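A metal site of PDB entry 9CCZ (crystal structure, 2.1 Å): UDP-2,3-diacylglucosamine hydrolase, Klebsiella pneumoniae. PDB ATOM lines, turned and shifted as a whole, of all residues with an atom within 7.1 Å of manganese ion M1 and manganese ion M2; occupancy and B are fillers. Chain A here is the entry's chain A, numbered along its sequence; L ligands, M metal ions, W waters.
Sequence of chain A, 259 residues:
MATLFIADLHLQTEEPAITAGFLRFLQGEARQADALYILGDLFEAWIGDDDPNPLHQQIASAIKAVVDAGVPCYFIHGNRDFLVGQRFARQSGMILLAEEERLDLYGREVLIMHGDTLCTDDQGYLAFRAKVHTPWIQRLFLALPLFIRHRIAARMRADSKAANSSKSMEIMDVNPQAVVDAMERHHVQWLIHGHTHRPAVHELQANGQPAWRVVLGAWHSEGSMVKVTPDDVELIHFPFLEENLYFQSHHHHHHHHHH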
ATOM      1  N   ALA A   7     -15.204  33.566  21.553  1.00  0.00           N
ATOM      2  CA  ALA A   7     -15.007  32.629  22.666  1.00  0.00           C
ATOM      3  C   ALA A   7     -15.445  31.239  22.219  1.00  0.00           C
ATOM      4  O   ALA A   7     -16.119  31.074  21.199  1.00  0.00           O
ATOM      5  CB  ALA A   7     -15.776  33.053  23.922  1.00  0.00           C
ATOM      6  N   ASP A   8     -15.040  30.241  23.004  1.00  0.00           N
ATOM      7  CA  ASP A   8     -15.538  28.872  22.871  1.00  0.00           C
ATOM      8  C   ASP A   8     -15.301  28.328  21.470  1.00  0.00           C
ATOM      9  O   ASP A   8     -16.181  27.702  20.869  1.00  0.00           O
ATOM     10  CB  ASP A   8     -17.016  28.802  23.263  1.00  0.00           C
ATOM     11  CG  ASP A   8     -17.241  29.206  24.697  1.00  0.00           C
ATOM     12  OD1 ASP A   8     -16.783  28.458  25.591  1.00  0.00           O
ATOM     13  OD2 ASP A   8     -17.826  30.274  24.940  1.00  0.00           O
ATOM     14  N   LEU A   9     -14.103  28.566  20.945  1.00  0.00           N
ATOM     15  CA  LEU A   9     -13.698  27.925  19.694  1.00  0.00           C
ATOM     16  C   LEU A   9     -13.365  26.449  19.908  1.00  0.00           C
ATOM     17  O   LEU A   9     -13.582  25.636  19.007  1.00  0.00           O
ATOM     18  CB  LEU A   9     -12.511  28.670  19.092  1.00  0.00           C
ATOM     19  CG  LEU A   9     -12.812  30.023  18.444  1.00  0.00           C
ATOM     20  CD1 LEU A   9     -12.850  31.147  19.475  1.00  0.00           C
ATOM     21  CD2 LEU A   9     -11.796  30.319  17.361  1.00  0.00           C
ATOM     22  N   HIS A  10     -12.869  26.097  21.088  1.00  0.00           N
ATOM     23  CA  HIS A  10     -12.498  24.722  21.421  1.00  0.00           C
ATOM     24  C   HIS A  10     -11.622  24.108  20.319  1.00  0.00           C
ATOM     25  O   HIS A  10     -11.882  22.998  19.833  1.00  0.00           O
ATOM     26  CB  HIS A  10     -13.739  23.860  21.666  1.00  0.00           C
ATOM     27  CG  HIS A  10     -14.591  24.325  22.807  1.00  0.00           C
ATOM     28  ND1 HIS A  10     -14.475  23.802  24.081  1.00  0.00           N
ATOM     29  CD2 HIS A  10     -15.561  25.271  22.873  1.00  0.00           C
ATOM     30  CE1 HIS A  10     -15.351  24.403  24.869  1.00  0.00           C
ATOM     31  NE2 HIS A  10     -16.018  25.293  24.166  1.00  0.00           N
ATOM     32  N   LEU A  39     -12.555  35.479  24.920  1.00  0.00           N
ATOM     33  CA  LEU A  39     -13.084  35.285  26.272  1.00  0.00           C
ATOM     34  C   LEU A  39     -13.110  33.814  26.680  1.00  0.00           C
ATOM     35  O   LEU A  39     -14.112  33.323  27.196  1.00  0.00           O
ATOM     36  CB  LEU A  39     -14.476  35.905  26.374  1.00  0.00           C
ATOM     37  CG  LEU A  39     -14.601  37.380  25.984  1.00  0.00           C
ATOM     38  CD1 LEU A  39     -15.990  37.919  26.317  1.00  0.00           C
ATOM     39  CD2 LEU A  39     -13.526  38.219  26.652  1.00  0.00           C
ATOM     40  N   GLY A  40     -12.020  33.095  26.437  1.00  0.00           N
ATOM     41  CA  GLY A  40     -11.849  31.784  27.037  1.00  0.00           C
ATOM     42  C   GLY A  40     -12.318  30.653  26.137  1.00  0.00           C
ATOM     43  O   GLY A  40     -13.126  30.834  25.217  1.00  0.00           O
ATOM     44  N   ASP A  41     -11.810  29.456  26.436  1.00  0.00           N
ATOM     45  CA  ASP A  41     -12.067  28.253  25.649  1.00  0.00           C
ATOM     46  C   ASP A  41     -11.642  28.446  24.196  1.00  0.00           C
ATOM     47  O   ASP A  41     -12.311  27.988  23.261  1.00  0.00           O
ATOM     48  CB  ASP A  41     -13.531  27.825  25.733  1.00  0.00           C
ATOM     49  CG  ASP A  41     -13.893  27.223  27.080  1.00  0.00           C
ATOM     50  OD1 ASP A  41     -12.992  27.119  27.958  1.00  0.00           O
ATOM     51  OD2 ASP A  41     -15.069  26.843  27.274  1.00  0.00           O
ATOM     52  N   GLU A  44      -9.661  23.419  23.162  1.00  0.00           N
ATOM     53  CA  GLU A  44     -10.427  22.390  23.855  1.00  0.00           C
ATOM     54  C   GLU A  44      -9.704  21.902  25.103  1.00  0.00           C
ATOM     55  O   GLU A  44     -10.345  21.445  26.053  1.00  0.00           O
ATOM     56  CB  GLU A  44     -10.705  21.223  22.909  1.00  0.00           C
ATOM     57  CG  GLU A  44     -11.339  19.986  23.560  1.00  0.00           C
ATOM     58  CD  GLU A  44     -12.745  20.239  24.100  1.00  0.00           C
ATOM     59  OE1 GLU A  44     -13.329  21.296  23.811  1.00  0.00           O
ATOM     60  OE2 GLU A  44     -13.254  19.372  24.842  1.00  0.00           O
ATOM     61  N   GLY A  78     -10.696  30.429  29.886  1.00  0.00           N
ATOM     62  CA  GLY A  78     -11.895  29.634  30.006  1.00  0.00           C
ATOM     63  C   GLY A  78     -11.699  28.473  30.957  1.00  0.00           C
ATOM     64  O   GLY A  78     -10.655  28.318  31.588  1.00  0.00           O
ATOM     65  N   ASN A  79     -12.735  27.631  31.052  1.00  0.00           N
ATOM     66  CA  ASN A  79     -12.626  26.453  31.897  1.00  0.00           C
ATOM     67  C   ASN A  79     -11.796  25.346  31.256  1.00  0.00           C
ATOM     68  O   ASN A  79     -11.276  24.488  31.980  1.00  0.00           O
ATOM     69  CB  ASN A  79     -14.028  25.925  32.262  1.00  0.00           C
ATOM     70  CG  ASN A  79     -14.870  25.588  31.050  1.00  0.00           C
ATOM     71  OD1 ASN A  79     -15.251  26.474  30.285  1.00  0.00           O
ATOM     72  ND2 ASN A  79     -15.189  24.320  30.881  1.00  0.00           N
ATOM     73  N   ARG A  80     -11.641  25.358  29.937  1.00  0.00           N
ATOM     74  CA  ARG A  80     -10.835  24.349  29.275  1.00  0.00           C
ATOM     75  C   ARG A  80      -9.357  24.729  29.227  1.00  0.00           C
ATOM     76  O   ARG A  80      -8.494  23.853  29.380  1.00  0.00           O
ATOM     77  CB  ARG A  80     -11.350  24.121  27.851  1.00  0.00           C
ATOM     78  CG  ARG A  80     -12.833  23.794  27.760  1.00  0.00           C
ATOM     79  CD  ARG A  80     -13.174  22.520  28.496  1.00  0.00           C
ATOM     80  NE  ARG A  80     -12.474  21.359  27.943  1.00  0.00           N
ATOM     81  CZ  ARG A  80     -12.745  20.099  28.252  1.00  0.00           C
ATOM     82  NH1 ARG A  80     -13.715  19.787  29.091  1.00  0.00           N
ATOM     83  NH2 ARG A  80     -12.036  19.125  27.687  1.00  0.00           N
ATOM     84  N   HIS A 114     -15.418  34.875  31.009  1.00  0.00           N
ATOM     85  CA  HIS A 114     -15.734  33.661  30.278  1.00  0.00           C
ATOM     86  C   HIS A 114     -17.182  33.241  30.526  1.00  0.00           C
ATOM     87  O   HIS A 114     -17.866  32.783  29.610  1.00  0.00           O
ATOM     88  CB  HIS A 114     -14.777  32.535  30.654  1.00  0.00           C
ATOM     89  CG  HIS A 114     -15.094  31.240  29.966  1.00  0.00           C
ATOM     90  ND1 HIS A 114     -15.041  31.097  28.595  1.00  0.00           N
ATOM     91  CD2 HIS A 114     -15.493  30.041  30.453  1.00  0.00           C
ATOM     92  CE1 HIS A 114     -15.391  29.866  28.269  1.00  0.00           C
ATOM     93  NE2 HIS A 114     -15.668  29.206  29.381  1.00  0.00           N
ATOM     94  N   GLY A 115     -17.645  33.390  31.768  1.00  0.00           N
ATOM     95  CA  GLY A 115     -19.024  33.088  32.122  1.00  0.00           C
ATOM     96  C   GLY A 115     -19.189  31.899  33.040  1.00  0.00           C
ATOM     97  O   GLY A 115     -20.294  31.719  33.581  1.00  0.00           O
ATOM     98  N   ASP A 116     -18.155  31.083  33.236  1.00  0.00           N
ATOM     99  CA  ASP A 116     -18.329  29.874  34.037  1.00  0.00           C
ATOM    100  C   ASP A 116     -18.522  30.199  35.515  1.00  0.00           C
ATOM    101  O   ASP A 116     -19.150  29.414  36.239  1.00  0.00           O
ATOM    102  CB  ASP A 116     -17.149  28.924  33.853  1.00  0.00           C
ATOM    103  CG  ASP A 116     -15.832  29.532  34.299  1.00  0.00           C
ATOM    104  OD1 ASP A 116     -15.520  30.659  33.874  1.00  0.00           O
ATOM    105  OD2 ASP A 116     -15.117  28.879  35.096  1.00  0.00           O
ATOM    106  N   TYR A 125     -19.233  21.166  39.147  1.00  0.00           N
ATOM    107  CA  TYR A 125     -18.240  21.900  38.375  1.00  0.00           C
ATOM    108  C   TYR A 125     -17.463  22.877  39.252  1.00  0.00           C
ATOM    109  O   TYR A 125     -16.232  22.989  39.121  1.00  0.00           O
ATOM    110  CB  TYR A 125     -18.890  22.664  37.219  1.00  0.00           C
ATOM    111  CG  TYR A 125     -17.952  23.690  36.648  1.00  0.00           C
ATOM    112  CD1 TYR A 125     -16.825  23.307  35.944  1.00  0.00           C
ATOM    113  CD2 TYR A 125     -18.173  25.049  36.849  1.00  0.00           C
ATOM    114  CE1 TYR A 125     -15.937  24.236  35.433  1.00  0.00           C
ATOM    115  CE2 TYR A 125     -17.292  25.993  36.340  1.00  0.00           C
ATOM    116  CZ  TYR A 125     -16.179  25.583  35.636  1.00  0.00           C
ATOM    117  OH  TYR A 125     -15.300  26.512  35.127  1.00  0.00           O
ATOM    118  N   ILE A 171     -24.030  21.686  29.375  1.00  0.00           N
ATOM    119  CA  ILE A 171     -23.489  22.803  30.143  1.00  0.00           C
ATOM    120  C   ILE A 171     -24.609  23.503  30.899  1.00  0.00           C
ATOM    121  O   ILE A 171     -25.618  23.887  30.306  1.00  0.00           O
ATOM    122  CB  ILE A 171     -22.736  23.785  29.237  1.00  0.00           C
ATOM    123  CG1 ILE A 171     -21.609  23.078  28.470  1.00  0.00           C
ATOM    124  CG2 ILE A 171     -22.168  24.945  30.053  1.00  0.00           C
ATOM    125  CD1 ILE A 171     -21.085  23.860  27.295  1.00  0.00           C
ATOM    126  N   GLY A 194     -19.181  33.996  27.436  1.00  0.00           N
ATOM    127  CA  GLY A 194     -19.426  32.814  26.642  1.00  0.00           C
ATOM    128  C   GLY A 194     -19.765  31.621  27.524  1.00  0.00           C
ATOM    129  O   GLY A 194     -20.695  31.698  28.343  1.00  0.00           O
ATOM    130  N   HIS A 195     -19.012  30.533  27.352  1.00  0.00           N
ATOM    131  CA  HIS A 195     -19.090  29.318  28.169  1.00  0.00           C
ATOM    132  C   HIS A 195     -20.383  28.523  27.968  1.00  0.00           C
ATOM    133  O   HIS A 195     -20.341  27.302  27.776  1.00  0.00           O
ATOM    134  CB  HIS A 195     -18.932  29.624  29.656  1.00  0.00           C
ATOM    135  CG  HIS A 195     -18.987  28.416  30.527  1.00  0.00           C
ATOM    136  ND1 HIS A 195     -18.026  27.427  30.487  1.00  0.00           N
ATOM    137  CD2 HIS A 195     -19.899  28.004  31.445  1.00  0.00           C
ATOM    138  CE1 HIS A 195     -18.333  26.475  31.344  1.00  0.00           C
ATOM    139  NE2 HIS A 195     -19.471  26.796  31.942  1.00  0.00           N
ATOM    140  N   THR A 196     -21.536  29.188  28.008  1.00  0.00           N
ATOM    141  CA  THR A 196     -22.805  28.464  27.968  1.00  0.00           C
ATOM    142  C   THR A 196     -23.188  27.995  26.571  1.00  0.00           C
ATOM    143  O   THR A 196     -24.105  27.174  26.446  1.00  0.00           O
ATOM    144  CB  THR A 196     -23.926  29.336  28.539  1.00  0.00           C
ATOM    145  OG1 THR A 196     -24.094  30.498  27.712  1.00  0.00           O
ATOM    146  CG2 THR A 196     -23.595  29.767  29.958  1.00  0.00           C
ATOM    147  N   HIS A 197     -22.522  28.491  25.526  1.00  0.00           N
ATOM    148  CA  HIS A 197     -22.802  28.079  24.141  1.00  0.00           C
ATOM    149  C   HIS A 197     -24.245  28.356  23.739  1.00  0.00           C
ATOM    150  O   HIS A 197     -24.816  27.649  22.904  1.00  0.00           O
ATOM    151  CB  HIS A 197     -22.455  26.598  23.923  1.00  0.00           C
ATOM    152  CG  HIS A 197     -21.019  26.252  24.195  1.00  0.00           C
ATOM    153  ND1 HIS A 197     -20.503  24.999  23.971  1.00  0.00           N
ATOM    154  CD2 HIS A 197     -19.992  27.005  24.653  1.00  0.00           C
ATOM    155  CE1 HIS A 197     -19.226  24.986  24.282  1.00  0.00           C
ATOM    156  NE2 HIS A 197     -18.888  26.191  24.703  1.00  0.00           N
ATOM    157  N   ALA A 218     -20.550  29.017  20.551  1.00  0.00           N
ATOM    158  CA  ALA A 218     -19.428  28.129  20.306  1.00  0.00           C
ATOM    159  C   ALA A 218     -19.270  27.881  18.814  1.00  0.00           C
ATOM    160  O   ALA A 218     -20.247  27.895  18.053  1.00  0.00           O
ATOM    161  CB  ALA A 218     -19.623  26.793  21.033  1.00  0.00           C
ATOM    162  N   HIS A 220     -19.130  25.467  16.575  1.00  0.00           N
ATOM    163  CA  HIS A 220     -19.421  24.068  16.278  1.00  0.00           C
ATOM    164  C   HIS A 220     -19.542  23.851  14.770  1.00  0.00           C
ATOM    165  O   HIS A 220     -18.785  23.080  14.179  1.00  0.00           O
ATOM    166  CB  HIS A 220     -20.700  23.626  17.003  1.00  0.00           C
ATOM    167  CG  HIS A 220     -20.525  23.402  18.477  1.00  0.00           C
ATOM    168  ND1 HIS A 220     -21.499  23.700  19.394  1.00  0.00           N
ATOM    169  CD2 HIS A 220     -19.484  22.899  19.175  1.00  0.00           C
ATOM    170  CE1 HIS A 220     -21.072  23.397  20.608  1.00  0.00           C
ATOM    171  NE2 HIS A 220     -19.851  22.907  20.505  1.00  0.00           N
HETATM  172  N1  LIG L   1      -5.588  19.374  34.032  1.00  0.00           N
HETATM  173  C1  LIG L   1      -5.673  18.131  33.292  1.00  0.00           C
HETATM  174  C2  LIG L   1      -5.409  20.517  33.150  1.00  0.00           C
HETATM  175  C3  LIG L   1      -9.491  19.714  30.861  1.00  0.00           C
HETATM  176  C4  LIG L   1     -10.233  18.627  31.325  1.00  0.00           C
HETATM  177  C5  LIG L   1     -12.004  20.136  31.985  1.00  0.00           C
HETATM  178  C6  LIG L   1      -9.987  21.016  30.970  1.00  0.00           C
HETATM  179  C7  LIG L   1     -14.190  21.220  32.938  1.00  0.00           C
HETATM  180  C8  LIG L   1      -4.544  20.790  37.128  1.00  0.00           C
HETATM  181  C9  LIG L   1      -5.213  19.452  35.413  1.00  0.00           C
HETATM  182  C10 LIG L   1      -5.191  18.333  36.211  1.00  0.00           C
HETATM  183  C11 LIG L   1      -4.813  18.465  37.531  1.00  0.00           C
HETATM  184  C12 LIG L   1      -4.485  19.723  38.017  1.00  0.00           C
HETATM  185  C13 LIG L   1      -4.766  17.240  38.450  1.00  0.00           C
HETATM  186  C14 LIG L   1      -6.875  18.222  32.361  1.00  0.00           C
HETATM  187  C15 LIG L   1      -6.576  20.612  32.191  1.00  0.00           C
HETATM  188  C16 LIG L   1     -11.506  18.848  31.877  1.00  0.00           C
HETATM  189  C17 LIG L   1     -11.240  21.227  31.524  1.00  0.00           C
HETATM  190  C18 LIG L   1     -15.557  20.989  33.580  1.00  0.00           C
HETATM  191  C19 LIG L   1     -13.720  18.691  32.841  1.00  0.00           C
HETATM  192  C20 LIG L   1     -12.522  17.867  32.447  1.00  0.00           C
HETATM  193  F1  LIG L   1      -5.827  17.234  39.275  1.00  0.00           F
HETATM  194  F2  LIG L   1      -3.637  17.274  39.177  1.00  0.00           F
HETATM  195  F3  LIG L   1      -4.776  16.116  37.706  1.00  0.00           F
HETATM  196  N2  LIG L   1      -4.896  20.634  35.887  1.00  0.00           N
HETATM  197  N3  LIG L   1      -6.792  19.363  31.471  1.00  0.00           N
HETATM  198  N4  LIG L   1     -13.355  20.083  32.605  1.00  0.00           N
HETATM  199  O1  LIG L   1      -7.462  20.522  29.254  1.00  0.00           O
HETATM  200  O2  LIG L   1      -7.803  18.231  29.327  1.00  0.00           O
HETATM  201  O3  LIG L   1     -13.805  22.323  32.713  1.00  0.00           O
HETATM  202  S1  LIG L   1      -7.856  19.436  30.159  1.00  0.00           S
HETATM  203 CL1  LIG L   1      -4.129  22.434  37.664  1.00  0.00          CL
HETATM  204 MN    MN M   1     -16.946  26.548  25.795  1.00  0.00          MN
HETATM  205 MN    MN M   2     -16.373  27.234  28.962  1.00  0.00          MN
HETATM  206  O   HOH W   1     -16.697  23.894  28.190  1.00  0.00           O
HETATM  207  O   HOH W   2     -17.376  26.370  27.535  1.00  0.00           O
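Of the 22 residues printed, 4 come within 4 Å of manganese ion M1.
Manganese ion M1 is bound by water W2 (1.8 Å), OD1 of Asp 8 (1.9 Å), NE2 of His 197 (2.3 Å), NE2 of His 10 (2.3 Å) and OD2 of Asp 41 (2.4 Å).
Manganese ion M2 is bound by OD1 of Asn 79 (1.9 Å), water W2 (1.9 Å), NE2 of His 114 (2.1 Å), OD2 of Asp 41 (2.2 Å) and ND1 of His 195 (2.3 Å).
Manganese ion M2 has five donor atoms within binding distance.
Of the 22 residues printed, 5 come within 4 Å of manganese ion M2.
The nearest printed residue that does not touch manganese ion M2 is His 197 (5.1 Å).
The side-chain carboxylate (OD2) of Asp 8 lies within hydrogen-bond range of the backbone NH (N) of His 195 (2.7 Å).
O of Gly 40 sits at hydrogen-bond distance from N of Asp 8 (3.0 Å).
O of His 114 is in hydrogen-bond range of N of Gly 194 (2.8 Å).
ND1 of His 114 lies within hydrogen-bond range of O of Leu 39 (2.8 Å).
OD1 of Asp 41 is in hydrogen-bond range of N of Arg 80, 3.0 Å away.
The backbone carbonyl oxygen (O) of Asp 41 is in hydrogen-bond range of the backbone NH (N) of Leu 9 (3.0 Å).
The side-chain carboxylate (OE1) of Glu 44 sits at hydrogen-bond distance from a ring nitrogen (ND1) of His 10, 2.8 Å away.
ND2 of Asn 79 is in hydrogen-bond range of O3 of the ligand, 3.0 Å away.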
